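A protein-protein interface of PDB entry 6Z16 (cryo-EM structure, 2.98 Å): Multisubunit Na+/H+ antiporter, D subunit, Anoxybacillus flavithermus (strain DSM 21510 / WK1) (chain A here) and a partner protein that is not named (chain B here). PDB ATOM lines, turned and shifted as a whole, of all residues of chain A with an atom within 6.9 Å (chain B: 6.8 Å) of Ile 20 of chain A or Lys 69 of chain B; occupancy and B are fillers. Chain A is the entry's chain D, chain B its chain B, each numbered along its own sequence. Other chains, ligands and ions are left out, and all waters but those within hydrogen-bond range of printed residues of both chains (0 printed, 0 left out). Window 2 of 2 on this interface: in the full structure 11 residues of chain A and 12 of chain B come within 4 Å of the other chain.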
ATOM      1  N   THR A  15      11.578   4.969  17.439  1.00  0.00           N
ATOM      2  CA  THR A  15      12.382   3.876  17.971  1.00  0.00           C
ATOM      3  C   THR A  15      13.427   4.396  18.934  1.00  0.00           C
ATOM      4  O   THR A  15      13.523   3.910  20.068  1.00  0.00           O
ATOM      5  CB  THR A  15      13.047   3.117  16.834  1.00  0.00           C
ATOM      6  OG1 THR A  15      12.038   2.653  15.935  1.00  0.00           O
ATOM      7  CG2 THR A  15      13.825   1.938  17.379  1.00  0.00           C
ATOM      8  N   ALA A  16      14.115   5.477  18.540  1.00  0.00           N
ATOM      9  CA  ALA A  16      15.147   6.066  19.382  1.00  0.00           C
ATOM     10  C   ALA A  16      14.560   6.544  20.696  1.00  0.00           C
ATOM     11  O   ALA A  16      15.124   6.270  21.765  1.00  0.00           O
ATOM     12  CB  ALA A  16      15.827   7.215  18.647  1.00  0.00           C
ATOM     13  N   ILE A  17      13.346   7.108  20.635  1.00  0.00           N
ATOM     14  CA  ILE A  17      12.689   7.605  21.834  1.00  0.00           C
ATOM     15  C   ILE A  17      12.365   6.453  22.769  1.00  0.00           C
ATOM     16  O   ILE A  17      12.724   6.486  23.954  1.00  0.00           O
ATOM     17  CB  ILE A  17      11.438   8.409  21.453  1.00  0.00           C
ATOM     18  CG1 ILE A  17      11.834   9.608  20.597  1.00  0.00           C
ATOM     19  CG2 ILE A  17      10.742   8.884  22.687  1.00  0.00           C
ATOM     20  CD1 ILE A  17      10.670  10.278  19.921  1.00  0.00           C
ATOM     21  N   VAL A  18      11.828   5.353  22.231  1.00  0.00           N
ATOM     22  CA  VAL A  18      11.468   4.267  23.137  1.00  0.00           C
ATOM     23  C   VAL A  18      12.675   3.442  23.528  1.00  0.00           C
ATOM     24  O   VAL A  18      12.548   2.557  24.376  1.00  0.00           O
ATOM     25  CB  VAL A  18      10.378   3.336  22.577  1.00  0.00           C
ATOM     26  CG1 VAL A  18       9.134   4.125  22.241  1.00  0.00           C
ATOM     27  CG2 VAL A  18      10.870   2.556  21.392  1.00  0.00           C
ATOM     28  N   LEU A  19      13.850   3.722  22.968  1.00  0.00           N
ATOM     29  CA  LEU A  19      15.022   3.043  23.486  1.00  0.00           C
ATOM     30  C   LEU A  19      15.625   3.778  24.668  1.00  0.00           C
ATOM     31  O   LEU A  19      16.566   3.263  25.278  1.00  0.00           O
ATOM     32  CB  LEU A  19      16.056   2.854  22.375  1.00  0.00           C
ATOM     33  CG  LEU A  19      15.674   1.814  21.318  1.00  0.00           C
ATOM     34  CD1 LEU A  19      16.582   1.883  20.103  1.00  0.00           C
ATOM     35  CD2 LEU A  19      15.703   0.428  21.924  1.00  0.00           C
ATOM     36  N   ILE A  20      15.088   4.949  25.021  1.00  0.00           N
ATOM     37  CA  ILE A  20      15.634   5.691  26.152  1.00  0.00           C
ATOM     38  C   ILE A  20      15.196   5.070  27.482  1.00  0.00           C
ATOM     39  O   ILE A  20      15.945   5.111  28.466  1.00  0.00           O
ATOM     40  CB  ILE A  20      15.227   7.172  26.015  1.00  0.00           C
ATOM     41  CG1 ILE A  20      15.786   7.740  24.713  1.00  0.00           C
ATOM     42  CG2 ILE A  20      15.750   8.022  27.159  1.00  0.00           C
ATOM     43  CD1 ILE A  20      15.289   9.109  24.373  1.00  0.00           C
ATOM     44  N   PHE A  21      14.027   4.419  27.512  1.00  0.00           N
ATOM     45  CA  PHE A  21      13.414   4.000  28.771  1.00  0.00           C
ATOM     46  C   PHE A  21      14.147   2.835  29.429  1.00  0.00           C
ATOM     47  O   PHE A  21      14.212   2.763  30.658  1.00  0.00           O
ATOM     48  CB  PHE A  21      11.954   3.624  28.545  1.00  0.00           C
ATOM     49  CG  PHE A  21      11.067   4.781  28.225  1.00  0.00           C
ATOM     50  CD1 PHE A  21      10.624   5.624  29.224  1.00  0.00           C
ATOM     51  CD2 PHE A  21      10.644   5.005  26.933  1.00  0.00           C
ATOM     52  CE1 PHE A  21       9.798   6.681  28.935  1.00  0.00           C
ATOM     53  CE2 PHE A  21       9.815   6.063  26.639  1.00  0.00           C
ATOM     54  CZ  PHE A  21       9.389   6.895  27.641  1.00  0.00           C
ATOM     55  N   PHE A  22      14.693   1.903  28.647  1.00  0.00           N
ATOM     56  CA  PHE A  22      15.329   0.702  29.193  1.00  0.00           C
ATOM     57  C   PHE A  22      16.780   0.591  28.724  1.00  0.00           C
ATOM     58  O   PHE A  22      17.085  -0.091  27.739  1.00  0.00           O
ATOM     59  CB  PHE A  22      14.496  -0.554  28.894  1.00  0.00           C
ATOM     60  CG  PHE A  22      13.970  -0.672  27.467  1.00  0.00           C
ATOM     61  CD1 PHE A  22      12.759  -0.101  27.112  1.00  0.00           C
ATOM     62  CD2 PHE A  22      14.624  -1.443  26.522  1.00  0.00           C
ATOM     63  CE1 PHE A  22      12.265  -0.224  25.828  1.00  0.00           C
ATOM     64  CE2 PHE A  22      14.140  -1.563  25.244  1.00  0.00           C
ATOM     65  CZ  PHE A  22      12.960  -0.955  24.894  1.00  0.00           C
ATOM     66  N   PRO A  23      17.712   1.258  29.413  1.00  0.00           N
ATOM     67  CA  PRO A  23      19.124   1.142  29.027  1.00  0.00           C
ATOM     68  C   PRO A  23      19.761  -0.177  29.429  1.00  0.00           C
ATOM     69  O   PRO A  23      20.506  -0.772  28.648  1.00  0.00           O
ATOM     70  CB  PRO A  23      19.783   2.308  29.770  1.00  0.00           C
ATOM     71  CG  PRO A  23      18.678   3.231  30.095  1.00  0.00           C
ATOM     72  CD  PRO A  23      17.510   2.354  30.370  1.00  0.00           C
ATOM     73  N   GLN A  29      16.727  -3.930  23.843  1.00  0.00           N
ATOM     74  CA  GLN A  29      17.355  -2.946  22.961  1.00  0.00           C
ATOM     75  C   GLN A  29      17.649  -3.549  21.594  1.00  0.00           C
ATOM     76  O   GLN A  29      17.273  -2.985  20.556  1.00  0.00           O
ATOM     77  CB  GLN A  29      18.655  -2.437  23.590  1.00  0.00           C
ATOM     78  CG  GLN A  29      18.528  -1.582  24.838  1.00  0.00           C
ATOM     79  CD  GLN A  29      18.104  -0.169  24.542  1.00  0.00           C
ATOM     80  OE1 GLN A  29      18.596   0.449  23.605  1.00  0.00           O
ATOM     81  NE2 GLN A  29      17.186   0.354  25.338  1.00  0.00           N
ATOM     82  N   TYR A 108      23.176   3.784  26.086  1.00  0.00           N
ATOM     83  CA  TYR A 108      22.360   4.476  25.082  1.00  0.00           C
ATOM     84  C   TYR A 108      22.914   4.376  23.665  1.00  0.00           C
ATOM     85  O   TYR A 108      22.681   5.270  22.858  1.00  0.00           O
ATOM     86  CB  TYR A 108      22.156   5.950  25.451  1.00  0.00           C
ATOM     87  CG  TYR A 108      21.362   6.141  26.711  1.00  0.00           C
ATOM     88  CD1 TYR A 108      19.979   6.173  26.683  1.00  0.00           C
ATOM     89  CD2 TYR A 108      22.000   6.245  27.937  1.00  0.00           C
ATOM     90  CE1 TYR A 108      19.257   6.330  27.836  1.00  0.00           C
ATOM     91  CE2 TYR A 108      21.287   6.397  29.093  1.00  0.00           C
ATOM     92  CZ  TYR A 108      19.920   6.441  29.037  1.00  0.00           C
ATOM     93  OH  TYR A 108      19.208   6.592  30.196  1.00  0.00           O
ATOM     94  N   SER A 111      20.163   4.049  20.758  1.00  0.00           N
ATOM     95  CA  SER A 111      19.471   5.320  20.591  1.00  0.00           C
ATOM     96  C   SER A 111      20.262   6.246  19.681  1.00  0.00           C
ATOM     97  O   SER A 111      19.704   6.851  18.763  1.00  0.00           O
ATOM     98  CB  SER A 111      19.257   5.974  21.952  1.00  0.00           C
ATOM     99  OG  SER A 111      18.492   5.148  22.801  1.00  0.00           O
ATOM    100  N   PHE A 115      19.310   7.803  16.083  1.00  0.00           N
ATOM    101  CA  PHE A 115      19.307   9.239  15.807  1.00  0.00           C
ATOM    102  C   PHE A 115      20.195   9.592  14.622  1.00  0.00           C
ATOM    103  O   PHE A 115      19.870  10.515  13.864  1.00  0.00           O
ATOM    104  CB  PHE A 115      19.734  10.057  17.028  1.00  0.00           C
ATOM    105  CG  PHE A 115      18.656  10.233  18.056  1.00  0.00           C
ATOM    106  CD1 PHE A 115      17.523  10.969  17.757  1.00  0.00           C
ATOM    107  CD2 PHE A 115      18.815   9.752  19.344  1.00  0.00           C
ATOM    108  CE1 PHE A 115      16.537  11.147  18.694  1.00  0.00           C
ATOM    109  CE2 PHE A 115      17.835   9.932  20.290  1.00  0.00           C
ATOM    110  CZ  PHE A 115      16.695  10.632  19.966  1.00  0.00           C
ATOM    111  N   ILE B  66      11.754  12.974  40.570  1.00  0.00           N
ATOM    112  CA  ILE B  66      11.692  12.702  39.141  1.00  0.00           C
ATOM    113  C   ILE B  66      13.091  12.316  38.678  1.00  0.00           C
ATOM    114  O   ILE B  66      14.083  12.876  39.159  1.00  0.00           O
ATOM    115  CB  ILE B  66      11.185  13.925  38.341  1.00  0.00           C
ATOM    116  CG1 ILE B  66       9.884  14.478  38.909  1.00  0.00           C
ATOM    117  CG2 ILE B  66      10.857  13.540  36.935  1.00  0.00           C
ATOM    118  CD1 ILE B  66       9.462  15.783  38.269  1.00  0.00           C
ATOM    119  N   ASN B  67      13.182  11.344  37.770  1.00  0.00           N
ATOM    120  CA  ASN B  67      14.336  11.250  36.889  1.00  0.00           C
ATOM    121  C   ASN B  67      13.993  11.894  35.549  1.00  0.00           C
ATOM    122  O   ASN B  67      12.870  11.778  35.053  1.00  0.00           O
ATOM    123  CB  ASN B  67      14.838   9.809  36.709  1.00  0.00           C
ATOM    124  CG  ASN B  67      13.772   8.838  36.238  1.00  0.00           C
ATOM    125  OD1 ASN B  67      12.606   9.179  36.074  1.00  0.00           O
ATOM    126  ND2 ASN B  67      14.190   7.606  35.993  1.00  0.00           N
ATOM    127  N   TYR B  68      14.962  12.602  34.987  1.00  0.00           N
ATOM    128  CA  TYR B  68      14.701  13.537  33.907  1.00  0.00           C
ATOM    129  C   TYR B  68      14.875  12.914  32.532  1.00  0.00           C
ATOM    130  O   TYR B  68      14.428  13.496  31.535  1.00  0.00           O
ATOM    131  CB  TYR B  68      15.613  14.752  34.079  1.00  0.00           C
ATOM    132  CG  TYR B  68      15.341  15.484  35.375  1.00  0.00           C
ATOM    133  CD1 TYR B  68      14.320  16.416  35.465  1.00  0.00           C
ATOM    134  CD2 TYR B  68      16.088  15.217  36.518  1.00  0.00           C
ATOM    135  CE1 TYR B  68      14.055  17.071  36.646  1.00  0.00           C
ATOM    136  CE2 TYR B  68      15.828  15.866  37.705  1.00  0.00           C
ATOM    137  CZ  TYR B  68      14.810  16.792  37.760  1.00  0.00           C
ATOM    138  OH  TYR B  68      14.552  17.445  38.939  1.00  0.00           O
ATOM    139  N   LYS B  69      15.493  11.735  32.469  1.00  0.00           N
ATOM    140  CA  LYS B  69      15.613  11.008  31.214  1.00  0.00           C
ATOM    141  C   LYS B  69      14.253  10.505  30.748  1.00  0.00           C
ATOM    142  O   LYS B  69      13.926  10.566  29.552  1.00  0.00           O
ATOM    143  CB  LYS B  69      16.617   9.876  31.403  1.00  0.00           C
ATOM    144  CG  LYS B  69      18.005  10.420  31.708  1.00  0.00           C
ATOM    145  CD  LYS B  69      19.068   9.361  31.878  1.00  0.00           C
ATOM    146  CE  LYS B  69      19.397   9.100  33.336  1.00  0.00           C
ATOM    147  NZ  LYS B  69      18.351   8.317  34.033  1.00  0.00           N
ATOM    148  N   TRP B  70      13.417  10.068  31.691  1.00  0.00           N
ATOM    149  CA  TRP B  70      12.039   9.762  31.343  1.00  0.00           C
ATOM    150  C   TRP B  70      11.274  11.011  30.939  1.00  0.00           C
ATOM    151  O   TRP B  70      10.399  10.930  30.082  1.00  0.00           O
ATOM    152  CB  TRP B  70      11.328   9.049  32.492  1.00  0.00           C
ATOM    153  CG  TRP B  70      11.790   7.636  32.717  1.00  0.00           C
ATOM    154  CD1 TRP B  70      12.761   6.972  32.030  1.00  0.00           C
ATOM    155  CD2 TRP B  70      11.248   6.696  33.649  1.00  0.00           C
ATOM    156  NE1 TRP B  70      12.886   5.690  32.504  1.00  0.00           N
ATOM    157  CE2 TRP B  70      11.962   5.493  33.493  1.00  0.00           C
ATOM    158  CE3 TRP B  70      10.238   6.759  34.611  1.00  0.00           C
ATOM    159  CZ2 TRP B  70      11.701   4.365  34.265  1.00  0.00           C
ATOM    160  CZ3 TRP B  70       9.978   5.638  35.376  1.00  0.00           C
ATOM    161  CH2 TRP B  70      10.707   4.457  35.198  1.00  0.00           C
ATOM    162  N   LEU B  71      11.622  12.178  31.492  1.00  0.00           N
ATOM    163  CA  LEU B  71      10.948  13.411  31.087  1.00  0.00           C
ATOM    164  C   LEU B  71      11.261  13.796  29.651  1.00  0.00           C
ATOM    165  O   LEU B  71      10.353  14.195  28.909  1.00  0.00           O
ATOM    166  CB  LEU B  71      11.306  14.572  32.006  1.00  0.00           C
ATOM    167  CG  LEU B  71      10.560  14.675  33.319  1.00  0.00           C
ATOM    168  CD1 LEU B  71      11.064  15.885  34.057  1.00  0.00           C
ATOM    169  CD2 LEU B  71       9.084  14.806  33.020  1.00  0.00           C
ATOM    170  N   VAL B  72      12.529  13.699  29.239  1.00  0.00           N
ATOM    171  CA  VAL B  72      12.848  14.066  27.861  1.00  0.00           C
ATOM    172  C   VAL B  72      12.267  13.049  26.883  1.00  0.00           C
ATOM    173  O   VAL B  72      11.757  13.425  25.814  1.00  0.00           O
ATOM    174  CB  VAL B  72      14.365  14.282  27.663  1.00  0.00           C
ATOM    175  CG1 VAL B  72      14.825  15.442  28.488  1.00  0.00           C
ATOM    176  CG2 VAL B  72      15.185  13.080  28.024  1.00  0.00           C
ATOM    177  N   ALA B  73      12.240  11.762  27.273  1.00  0.00           N
ATOM    178  CA  ALA B  73      11.630  10.746  26.418  1.00  0.00           C
ATOM    179  C   ALA B  73      10.126  10.966  26.261  1.00  0.00           C
ATOM    180  O   ALA B  73       9.599  10.910  25.143  1.00  0.00           O
ATOM    181  CB  ALA B  73      11.919   9.360  26.984  1.00  0.00           C
ATOM    182  N   ILE B  74       9.431  11.276  27.359  1.00  0.00           N
ATOM    183  CA  ILE B  74       7.985  11.465  27.313  1.00  0.00           C
ATOM    184  C   ILE B  74       7.614  12.763  26.590  1.00  0.00           C
ATOM    185  O   ILE B  74       6.602  12.810  25.881  1.00  0.00           O
ATOM    186  CB  ILE B  74       7.426  11.372  28.751  1.00  0.00           C
ATOM    187  CG1 ILE B  74       7.500   9.928  29.243  1.00  0.00           C
ATOM    188  CG2 ILE B  74       5.989  11.799  28.853  1.00  0.00           C
ATOM    189  CD1 ILE B  74       7.299   9.786  30.731  1.00  0.00           C
ATOM    190  N   LEU B  76       9.389  14.144  24.034  1.00  0.00           N
ATOM    191  CA  LEU B  76       9.540  13.724  22.642  1.00  0.00           C
ATOM    192  C   LEU B  76       8.341  12.904  22.169  1.00  0.00           C
ATOM    193  O   LEU B  76       7.843  13.109  21.051  1.00  0.00           O
ATOM    194  CB  LEU B  76      10.840  12.939  22.501  1.00  0.00           C
ATOM    195  CG  LEU B  76      12.120  13.768  22.553  1.00  0.00           C
ATOM    196  CD1 LEU B  76      13.321  12.908  22.853  1.00  0.00           C
ATOM    197  CD2 LEU B  76      12.290  14.410  21.205  1.00  0.00           C
ATOM    198  N   GLY B 127      14.030  18.640  31.377  1.00  0.00           N
ATOM    199  CA  GLY B 127      14.804  17.429  31.566  1.00  0.00           C
ATOM    200  C   GLY B 127      16.252  17.555  31.134  1.00  0.00           C
ATOM    201  O   GLY B 127      17.146  17.109  31.848  1.00  0.00           O
ATOM    202  N   ILE B 131      19.441  17.273  33.570  1.00  0.00           N
ATOM    203  CA  ILE B 131      20.407  16.196  33.328  1.00  0.00           C
ATOM    204  C   ILE B 131      21.822  16.750  33.286  1.00  0.00           C
ATOM    205  O   ILE B 131      22.722  16.222  33.947  1.00  0.00           O
ATOM    206  CB  ILE B 131      20.075  15.428  32.032  1.00  0.00           C
ATOM    207  CG1 ILE B 131      18.885  14.498  32.209  1.00  0.00           C
ATOM    208  CG2 ILE B 131      21.244  14.577  31.578  1.00  0.00           C
ATOM    209  CD1 ILE B 131      18.318  14.039  30.886  1.00  0.00           C
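Ile 17 of chain A touches Ala 73 of chain B (CG2 to O, 3.4 Å).
Leu 76 of chain B touches Ile 17 of chain A (CB to CD1, 3.7 Å).
Lys 69 of chain B touches Ile 20 of chain A.
O of Phe 21 of chain A touches NE1 of Trp 70 of chain B, at 3.7 Å.
CB of Ala 73 of chain B touches CZ of Phe 21 of chain A (3.6 Å).
CG1 of Ile 74 of chain B touches CZ of Phe 21 of chain A (3.9 Å).
Tyr 108 of chain A touches Lys 69 of chain B (OH to CD, 3.2 Å).
Of the 13 printed residues of chain A, 4 touch a printed residue of chain B.
Printed residues of chain A that touch a printed residue of chain B: Ile 17, Ile 20, Phe 21 and Tyr 108.
Hydrophobic or aromatic side chains of chain A that line the printed part of chain B: Ile 17, Ile 20, Phe 21 and Tyr 108.
Along chain A the printed residues that touch a printed residue of chain B span positions 17 to 108.
Hydrophobic or aromatic side chains of chain B that line the printed part of chain A: Trp 70, Ala 73, Ile 74 and Leu 76.
Among the printed residues, no Asp or Glu carboxylate lies within 4 Å of a Lys or Arg side-chain nitrogen of the other chain.
Of chain B, only Lys 69 comes within 4 Å of Ile 20 of chain A.
Lys 69 of chain B touches two residues of chain A.
Of the printed residues of chain A, Ile 74 of chain B touches Phe 21 (3.9 Å).
Of the printed residues of chain B, Phe 21 of chain A touches Trp 70 (3.7 Å), Ala 73 (3.6 Å) and Ile 74 (3.9 Å).
Printed residues of chain A within 4 Å of Leu 76 of chain B: Ile 17.
Ala 16 of chain A touches none of the printed residues of chain B.
The nearest residue of chain B that does not touch Ile 20 of chain A is Ala 73 of chain B (4.1 Å).
The nearest residue of chain A that does not touch Lys 69 of chain B is Phe 21 of chain A (5.7 Å).
The nearest printed residue of chain A that does not touch Leu 76 of chain B is Ile 20 of chain A (4.5 Å).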
